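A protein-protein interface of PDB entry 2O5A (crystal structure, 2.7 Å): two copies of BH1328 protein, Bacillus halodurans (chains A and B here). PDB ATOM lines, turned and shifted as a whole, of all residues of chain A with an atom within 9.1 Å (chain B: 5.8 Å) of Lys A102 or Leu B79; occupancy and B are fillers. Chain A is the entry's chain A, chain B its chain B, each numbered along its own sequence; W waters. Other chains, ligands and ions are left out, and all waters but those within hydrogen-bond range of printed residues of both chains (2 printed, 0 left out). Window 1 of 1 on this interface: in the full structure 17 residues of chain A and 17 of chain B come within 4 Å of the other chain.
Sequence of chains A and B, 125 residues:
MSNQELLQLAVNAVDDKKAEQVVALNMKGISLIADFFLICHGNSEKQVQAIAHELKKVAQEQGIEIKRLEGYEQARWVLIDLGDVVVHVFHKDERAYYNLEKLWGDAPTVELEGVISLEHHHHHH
Water W2 lies within hydrogen-bond range of the guanidinium group (NH1) of Arg B68 (2.7 Å), the side-chain carboxylate (OE1) of Glu A101 (2.8 Å) and the side-chain carboxylate (OE1) of Glu B70 (2.8 Å). Water W1 lies within hydrogen-bond range of the side-chain amino group (NZ) of Lys A102 (2.7 Å) and the backbone NH (N) of Gly B71 (2.9 Å).
No position is printed for both chains. Of the 7 pairs that touch across the chains among the printed residues, none has its exchanged pair printed and touching as well.
The guanidinium group of Arg B68 lies within salt-bridge range of the side-chain carboxylate of Asp B81. O of Glu B70 lies within hydrogen-bond range of N of Leu B79 (2.9 Å).
Trp B77 touches Asn A99 (CE3 to OD1, 3.2 Å). NZ of Lys A102 touches O of Glu B70, at 3.8 Å. Gly B71 touches Lys A102. Lys A102 touches Leu B79.
The backbone carbonyl oxygen (O) of Lys A102 lies within hydrogen-bond range of the guanidinium group (NH1) of Arg B68 (2.6 Å). O of Trp B77 sits close to NZ of Lys A102 (3.4 Å). The side-chain carboxylate (OE2) of Glu B70 lies close to the side-chain carboxylate (OE1) of Glu A101, at 3.3 Å.
Hydrophobic or aromatic side chains of chain B within 4 Å of the printed part of chain A: Trp B77 and Leu B79. Among the printed residues, no Asp or Glu carboxylate lies within 4 Å of a Lys or Arg side-chain nitrogen of the other chain.
Of the printed residues of chain B, Glu A101 touches Glu B70. Of chain B, only Arg B68 (2.6 Å), Glu B70 (3.8 Å), Gly B71 (3.9 Å), Trp B77 (3.3 Å) and Leu B79 (3.2 Å) come within 4 Å of Lys A102. Of the printed residues of chain A, Trp B77 touches Asn A99 (3.2 Å) and Lys A102 (3.3 Å). Val B78 touches none of the printed residues of chain A. No residue of chain A comes within 4 Å of Ile B80. His B88 touches none of the printed residues of chain A. Val B89 touches none of the printed residues of chain A. The nearest residue of chain A that does not touch Leu B79 is Leu A103 (4.7 Å).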
ATOM      1  N   ILE A  30       5.585  13.827  16.605  1.00  0.00           N
ATOM      2  CA  ILE A  30       6.816  14.358  16.042  1.00  0.00           C
ATOM      3  C   ILE A  30       8.035  13.622  16.560  1.00  0.00           C
ATOM      4  O   ILE A  30       8.880  13.179  15.784  1.00  0.00           O
ATOM      5  CB  ILE A  30       6.914  15.846  16.359  1.00  0.00           C
ATOM      6  CG1 ILE A  30       5.511  16.431  16.182  1.00  0.00           C
ATOM      7  CG2 ILE A  30       7.993  16.514  15.506  1.00  0.00           C
ATOM      8  CD1 ILE A  30       5.024  16.599  14.808  1.00  0.00           C
ATOM      9  N   ARG A  95      22.843  31.138  17.764  1.00  0.00           N
ATOM     10  CA  ARG A  95      22.218  31.130  16.444  1.00  0.00           C
ATOM     11  C   ARG A  95      21.194  30.020  16.220  1.00  0.00           C
ATOM     12  O   ARG A  95      20.143  30.257  15.626  1.00  0.00           O
ATOM     13  CB  ARG A  95      23.286  31.062  15.347  1.00  0.00           C
ATOM     14  CG  ARG A  95      24.146  32.312  15.242  1.00  0.00           C
ATOM     15  CD  ARG A  95      24.848  32.393  13.894  1.00  0.00           C
ATOM     16  NE  ARG A  95      25.887  31.380  13.739  1.00  0.00           N
ATOM     17  CZ  ARG A  95      26.612  31.218  12.636  1.00  0.00           C
ATOM     18  NH1 ARG A  95      26.410  32.003  11.586  1.00  0.00           N
ATOM     19  NH2 ARG A  95      27.544  30.279  12.584  1.00  0.00           N
ATOM     20  N   ALA A  96      21.499  28.812  16.681  1.00  0.00           N
ATOM     21  CA  ALA A  96      20.579  27.691  16.513  1.00  0.00           C
ATOM     22  C   ALA A  96      19.257  28.006  17.203  1.00  0.00           C
ATOM     23  O   ALA A  96      18.248  27.339  16.978  1.00  0.00           O
ATOM     24  CB  ALA A  96      21.184  26.421  17.096  1.00  0.00           C
ATOM     25  N   TYR A  97      19.279  29.037  18.041  1.00  0.00           N
ATOM     26  CA  TYR A  97      18.107  29.472  18.788  1.00  0.00           C
ATOM     27  C   TYR A  97      17.148  30.272  17.910  1.00  0.00           C
ATOM     28  O   TYR A  97      15.968  30.415  18.232  1.00  0.00           O
ATOM     29  CB  TYR A  97      18.557  30.307  19.993  1.00  0.00           C
ATOM     30  CG  TYR A  97      17.435  30.939  20.784  1.00  0.00           C
ATOM     31  CD1 TYR A  97      16.374  30.173  21.263  1.00  0.00           C
ATOM     32  CD2 TYR A  97      17.445  32.303  21.069  1.00  0.00           C
ATOM     33  CE1 TYR A  97      15.345  30.750  21.999  1.00  0.00           C
ATOM     34  CE2 TYR A  97      16.422  32.891  21.805  1.00  0.00           C
ATOM     35  CZ  TYR A  97      15.377  32.105  22.267  1.00  0.00           C
ATOM     36  OH  TYR A  97      14.352  32.676  22.985  1.00  0.00           O
ATOM     37  N   TYR A  98      17.659  30.790  16.796  1.00  0.00           N
ATOM     38  CA  TYR A  98      16.835  31.564  15.876  1.00  0.00           C
ATOM     39  C   TYR A  98      16.530  30.759  14.618  1.00  0.00           C
ATOM     40  O   TYR A  98      15.812  31.216  13.728  1.00  0.00           O
ATOM     41  CB  TYR A  98      17.533  32.878  15.516  1.00  0.00           C
ATOM     42  CG  TYR A  98      17.766  33.767  16.718  1.00  0.00           C
ATOM     43  CD1 TYR A  98      18.944  33.680  17.459  1.00  0.00           C
ATOM     44  CD2 TYR A  98      16.790  34.668  17.139  1.00  0.00           C
ATOM     45  CE1 TYR A  98      19.140  34.464  18.598  1.00  0.00           C
ATOM     46  CE2 TYR A  98      16.974  35.454  18.274  1.00  0.00           C
ATOM     47  CZ  TYR A  98      18.152  35.349  18.997  1.00  0.00           C
ATOM     48  OH  TYR A  98      18.331  36.119  20.124  1.00  0.00           O
ATOM     49  N   ASN A  99      17.085  29.553  14.563  1.00  0.00           N
ATOM     50  CA  ASN A  99      16.875  28.640  13.444  1.00  0.00           C
ATOM     51  C   ASN A  99      16.116  27.436  13.975  1.00  0.00           C
ATOM     52  O   ASN A  99      15.946  26.430  13.284  1.00  0.00           O
ATOM     53  CB  ASN A  99      18.216  28.194  12.860  1.00  0.00           C
ATOM     54  CG  ASN A  99      18.879  29.276  12.030  1.00  0.00           C
ATOM     55  OD1 ASN A  99      20.039  29.151  11.642  1.00  0.00           O
ATOM     56  ND2 ASN A  99      18.137  30.339  11.742  1.00  0.00           N
ATOM     57  N   LEU A 100      15.662  27.557  15.217  1.00  0.00           N
ATOM     58  CA  LEU A 100      14.914  26.501  15.876  1.00  0.00           C
ATOM     59  C   LEU A 100      13.579  26.338  15.161  1.00  0.00           C
ATOM     60  O   LEU A 100      12.759  25.494  15.522  1.00  0.00           O
ATOM     61  CB  LEU A 100      14.695  26.876  17.340  1.00  0.00           C
ATOM     62  CG  LEU A 100      14.984  25.785  18.369  1.00  0.00           C
ATOM     63  CD1 LEU A 100      16.295  25.088  18.044  1.00  0.00           C
ATOM     64  CD2 LEU A 100      15.041  26.405  19.747  1.00  0.00           C
ATOM     65  N   GLU A 101      13.379  27.162  14.138  1.00  0.00           N
ATOM     66  CA  GLU A 101      12.166  27.139  13.336  1.00  0.00           C
ATOM     67  C   GLU A 101      12.253  25.937  12.400  1.00  0.00           C
ATOM     68  O   GLU A 101      11.339  25.114  12.347  1.00  0.00           O
ATOM     69  CB  GLU A 101      12.057  28.445  12.541  1.00  0.00           C
ATOM     70  CG  GLU A 101      10.677  28.750  11.970  1.00  0.00           C
ATOM     71  CD  GLU A 101      10.475  28.209  10.569  1.00  0.00           C
ATOM     72  OE1 GLU A 101      10.537  26.976  10.386  1.00  0.00           O
ATOM     73  OE2 GLU A 101      10.251  29.022   9.647  1.00  0.00           O
ATOM     74  N   LYS A 102      13.363  25.841  11.671  1.00  0.00           N
ATOM     75  CA  LYS A 102      13.581  24.729  10.752  1.00  0.00           C
ATOM     76  C   LYS A 102      13.248  23.448  11.499  1.00  0.00           C
ATOM     77  O   LYS A 102      12.410  22.657  11.067  1.00  0.00           O
ATOM     78  CB  LYS A 102      15.043  24.688  10.300  1.00  0.00           C
ATOM     79  CG  LYS A 102      15.559  25.978   9.690  1.00  0.00           C
ATOM     80  CD  LYS A 102      16.959  25.786   9.129  1.00  0.00           C
ATOM     81  CE  LYS A 102      17.625  27.117   8.818  1.00  0.00           C
ATOM     82  NZ  LYS A 102      16.842  27.929   7.847  1.00  0.00           N
ATOM     83  N   LEU A 103      13.916  23.257  12.630  1.00  0.00           N
ATOM     84  CA  LEU A 103      13.691  22.092  13.470  1.00  0.00           C
ATOM     85  C   LEU A 103      12.289  22.158  14.042  1.00  0.00           C
ATOM     86  O   LEU A 103      11.745  23.240  14.243  1.00  0.00           O
ATOM     87  CB  LEU A 103      14.670  22.086  14.641  1.00  0.00           C
ATOM     88  CG  LEU A 103      16.169  22.061  14.362  1.00  0.00           C
ATOM     89  CD1 LEU A 103      16.909  22.619  15.562  1.00  0.00           C
ATOM     90  CD2 LEU A 103      16.614  20.644  14.057  1.00  0.00           C
ATOM     91  N   TRP A 104      11.716  21.004  14.350  1.00  0.00           N
ATOM     92  CA  TRP A 104      10.391  20.985  14.947  1.00  0.00           C
ATOM     93  C   TRP A 104       9.505  22.030  14.278  1.00  0.00           C
ATOM     94  O   TRP A 104       9.707  22.372  13.113  1.00  0.00           O
ATOM     95  CB  TRP A 104      10.518  21.275  16.450  1.00  0.00           C
ATOM     96  CG  TRP A 104      11.859  20.865  17.021  1.00  0.00           C
ATOM     97  CD1 TRP A 104      12.534  19.703  16.769  1.00  0.00           C
ATOM     98  CD2 TRP A 104      12.683  21.612  17.926  1.00  0.00           C
ATOM     99  NE1 TRP A 104      13.724  19.683  17.456  1.00  0.00           N
ATOM    100  CE2 TRP A 104      13.839  20.846  18.179  1.00  0.00           C
ATOM    101  CE3 TRP A 104      12.553  22.860  18.554  1.00  0.00           C
ATOM    102  CZ2 TRP A 104      14.867  21.277  19.024  1.00  0.00           C
ATOM    103  CZ3 TRP A 104      13.570  23.289  19.395  1.00  0.00           C
ATOM    104  CH2 TRP A 104      14.711  22.498  19.626  1.00  0.00           C
ATOM    105  N   PRO A 108       4.366  23.369  16.246  1.00  0.00           N
ATOM    106  CA  PRO A 108       3.166  23.145  17.058  1.00  0.00           C
ATOM    107  C   PRO A 108       3.412  23.467  18.531  1.00  0.00           C
ATOM    108  O   PRO A 108       3.896  22.626  19.287  1.00  0.00           O
ATOM    109  CB  PRO A 108       2.883  21.668  16.831  1.00  0.00           C
ATOM    110  CG  PRO A 108       4.263  21.096  16.757  1.00  0.00           C
ATOM    111  CD  PRO A 108       4.979  22.085  15.858  1.00  0.00           C
ATOM    112  N   ARG B  68       9.466  21.574   2.289  1.00  0.00           N
ATOM    113  CA  ARG B  68      10.095  22.783   2.799  1.00  0.00           C
ATOM    114  C   ARG B  68      11.453  23.064   2.173  1.00  0.00           C
ATOM    115  O   ARG B  68      12.135  22.163   1.688  1.00  0.00           O
ATOM    116  CB  ARG B  68      10.270  22.704   4.317  1.00  0.00           C
ATOM    117  CG  ARG B  68       9.027  23.013   5.129  1.00  0.00           C
ATOM    118  CD  ARG B  68       9.370  23.058   6.608  1.00  0.00           C
ATOM    119  NE  ARG B  68       9.793  21.751   7.106  1.00  0.00           N
ATOM    120  CZ  ARG B  68      10.534  21.570   8.193  1.00  0.00           C
ATOM    121  NH1 ARG B  68      10.944  22.611   8.904  1.00  0.00           N
ATOM    122  NH2 ARG B  68      10.861  20.344   8.578  1.00  0.00           N
ATOM    123  N   LEU B  69      11.827  24.337   2.196  1.00  0.00           N
ATOM    124  CA  LEU B  69      13.102  24.801   1.676  1.00  0.00           C
ATOM    125  C   LEU B  69      13.311  26.158   2.329  1.00  0.00           C
ATOM    126  O   LEU B  69      12.638  27.132   1.988  1.00  0.00           O
ATOM    127  CB  LEU B  69      13.061  24.935   0.154  1.00  0.00           C
ATOM    128  CG  LEU B  69      14.400  25.295  -0.496  1.00  0.00           C
ATOM    129  CD1 LEU B  69      14.460  24.719  -1.898  1.00  0.00           C
ATOM    130  CD2 LEU B  69      14.585  26.802  -0.511  1.00  0.00           C
ATOM    131  N   GLU B  70      14.236  26.213   3.280  1.00  0.00           N
ATOM    132  CA  GLU B  70      14.494  27.449   4.003  1.00  0.00           C
ATOM    133  C   GLU B  70      15.981  27.765   4.131  1.00  0.00           C
ATOM    134  O   GLU B  70      16.814  26.866   4.246  1.00  0.00           O
ATOM    135  CB  GLU B  70      13.859  27.358   5.393  1.00  0.00           C
ATOM    136  CG  GLU B  70      12.406  26.895   5.365  1.00  0.00           C
ATOM    137  CD  GLU B  70      11.801  26.747   6.748  1.00  0.00           C
ATOM    138  OE1 GLU B  70      10.676  26.215   6.851  1.00  0.00           O
ATOM    139  OE2 GLU B  70      12.446  27.169   7.730  1.00  0.00           O
ATOM    140  N   GLY B  71      16.298  29.057   4.104  1.00  0.00           N
ATOM    141  CA  GLY B  71      17.676  29.495   4.227  1.00  0.00           C
ATOM    142  C   GLY B  71      18.495  29.397   2.954  1.00  0.00           C
ATOM    143  O   GLY B  71      19.724  29.411   3.007  1.00  0.00           O
ATOM    144  N   TRP B  77      22.569  27.787   6.164  1.00  0.00           N
ATOM    145  CA  TRP B  77      21.914  26.572   6.623  1.00  0.00           C
ATOM    146  C   TRP B  77      20.628  26.391   5.829  1.00  0.00           C
ATOM    147  O   TRP B  77      19.576  26.908   6.201  1.00  0.00           O
ATOM    148  CB  TRP B  77      21.586  26.671   8.117  1.00  0.00           C
ATOM    149  CG  TRP B  77      20.916  25.447   8.678  1.00  0.00           C
ATOM    150  CD1 TRP B  77      20.550  24.320   7.999  1.00  0.00           C
ATOM    151  CD2 TRP B  77      20.524  25.236  10.042  1.00  0.00           C
ATOM    152  NE1 TRP B  77      19.954  23.425   8.852  1.00  0.00           N
ATOM    153  CE2 TRP B  77      19.924  23.962  10.107  1.00  0.00           C
ATOM    154  CE3 TRP B  77      20.621  26.005  11.208  1.00  0.00           C
ATOM    155  CZ2 TRP B  77      19.423  23.434  11.304  1.00  0.00           C
ATOM    156  CZ3 TRP B  77      20.122  25.478  12.395  1.00  0.00           C
ATOM    157  CH2 TRP B  77      19.531  24.206  12.433  1.00  0.00           C
ATOM    158  N   VAL B  78      20.725  25.649   4.731  1.00  0.00           N
ATOM    159  CA  VAL B  78      19.575  25.398   3.878  1.00  0.00           C
ATOM    160  C   VAL B  78      18.911  24.080   4.251  1.00  0.00           C
ATOM    161  O   VAL B  78      19.573  23.044   4.348  1.00  0.00           O
ATOM    162  CB  VAL B  78      19.986  25.344   2.395  1.00  0.00           C
ATOM    163  CG1 VAL B  78      18.751  25.259   1.517  1.00  0.00           C
ATOM    164  CG2 VAL B  78      20.809  26.574   2.045  1.00  0.00           C
ATOM    165  N   LEU B  79      17.601  24.126   4.461  1.00  0.00           N
ATOM    166  CA  LEU B  79      16.842  22.936   4.816  1.00  0.00           C
ATOM    167  C   LEU B  79      15.896  22.586   3.676  1.00  0.00           C
ATOM    168  O   LEU B  79      15.092  23.412   3.249  1.00  0.00           O
ATOM    169  CB  LEU B  79      16.051  23.182   6.109  1.00  0.00           C
ATOM    170  CG  LEU B  79      15.232  22.027   6.696  1.00  0.00           C
ATOM    171  CD1 LEU B  79      14.905  22.326   8.142  1.00  0.00           C
ATOM    172  CD2 LEU B  79      13.958  21.817   5.895  1.00  0.00           C
ATOM    173  N   ILE B  80      16.007  21.359   3.178  1.00  0.00           N
ATOM    174  CA  ILE B  80      15.160  20.891   2.092  1.00  0.00           C
ATOM    175  C   ILE B  80      14.350  19.701   2.588  1.00  0.00           C
ATOM    176  O   ILE B  80      14.878  18.602   2.744  1.00  0.00           O
ATOM    177  CB  ILE B  80      16.002  20.445   0.877  1.00  0.00           C
ATOM    178  CG1 ILE B  80      16.989  21.549   0.498  1.00  0.00           C
ATOM    179  CG2 ILE B  80      15.090  20.138  -0.303  1.00  0.00           C
ATOM    180  CD1 ILE B  80      17.961  21.906   1.600  1.00  0.00           C
ATOM    181  N   ASP B  81      13.066  19.932   2.843  1.00  0.00           N
ATOM    182  CA  ASP B  81      12.188  18.876   3.334  1.00  0.00           C
ATOM    183  C   ASP B  81      11.634  18.066   2.167  1.00  0.00           C
ATOM    184  O   ASP B  81      10.803  18.556   1.401  1.00  0.00           O
ATOM    185  CB  ASP B  81      11.029  19.490   4.124  1.00  0.00           C
ATOM    186  CG  ASP B  81      10.366  18.490   5.048  1.00  0.00           C
ATOM    187  OD1 ASP B  81      10.421  17.278   4.758  1.00  0.00           O
ATOM    188  OD2 ASP B  81       9.777  18.919   6.062  1.00  0.00           O
ATOM    189  N   VAL B  86      14.930  14.477   5.114  1.00  0.00           N
ATOM    190  CA  VAL B  86      15.136  15.907   5.276  1.00  0.00           C
ATOM    191  C   VAL B  86      16.630  16.169   5.168  1.00  0.00           C
ATOM    192  O   VAL B  86      17.420  15.621   5.935  1.00  0.00           O
ATOM    193  CB  VAL B  86      14.630  16.399   6.651  1.00  0.00           C
ATOM    194  CG1 VAL B  86      15.026  17.853   6.861  1.00  0.00           C
ATOM    195  CG2 VAL B  86      13.116  16.248   6.730  1.00  0.00           C
ATOM    196  N   VAL B  87      17.012  17.000   4.208  1.00  0.00           N
ATOM    197  CA  VAL B  87      18.418  17.309   3.997  1.00  0.00           C
ATOM    198  C   VAL B  87      18.822  18.647   4.598  1.00  0.00           C
ATOM    199  O   VAL B  87      18.108  19.643   4.472  1.00  0.00           O
ATOM    200  CB  VAL B  87      18.762  17.332   2.494  1.00  0.00           C
ATOM    201  CG1 VAL B  87      20.272  17.340   2.308  1.00  0.00           C
ATOM    202  CG2 VAL B  87      18.140  16.132   1.798  1.00  0.00           C
ATOM    203  N   HIS B  88      19.979  18.655   5.253  1.00  0.00           N
ATOM    204  CA  HIS B  88      20.518  19.861   5.864  1.00  0.00           C
ATOM    205  C   HIS B  88      21.857  20.193   5.217  1.00  0.00           C
ATOM    206  O   HIS B  88      22.842  19.484   5.415  1.00  0.00           O
ATOM    207  CB  HIS B  88      20.720  19.662   7.367  1.00  0.00           C
ATOM    208  CG  HIS B  88      19.443  19.601   8.148  1.00  0.00           C
ATOM    209  ND1 HIS B  88      18.649  18.478   8.193  1.00  0.00           N
ATOM    210  CD2 HIS B  88      18.834  20.525   8.928  1.00  0.00           C
ATOM    211  CE1 HIS B  88      17.603  18.710   8.967  1.00  0.00           C
ATOM    212  NE2 HIS B  88      17.696  19.946   9.429  1.00  0.00           N
ATOM    213  N   VAL B  89      21.887  21.268   4.438  1.00  0.00           N
ATOM    214  CA  VAL B  89      23.110  21.687   3.764  1.00  0.00           C
ATOM    215  C   VAL B  89      23.687  22.902   4.474  1.00  0.00           C
ATOM    216  O   VAL B  89      23.175  24.014   4.333  1.00  0.00           O
ATOM    217  CB  VAL B  89      22.839  22.053   2.286  1.00  0.00           C
ATOM    218  CG1 VAL B  89      24.149  22.394   1.582  1.00  0.00           C
ATOM    219  CG2 VAL B  89      22.140  20.899   1.584  1.00  0.00           C
HETATM  220  O   HOH W   1      15.531  30.013   6.758  1.00  0.00           O
HETATM  221  O   HOH W   2       9.467  24.838   9.008  1.00  0.00           O
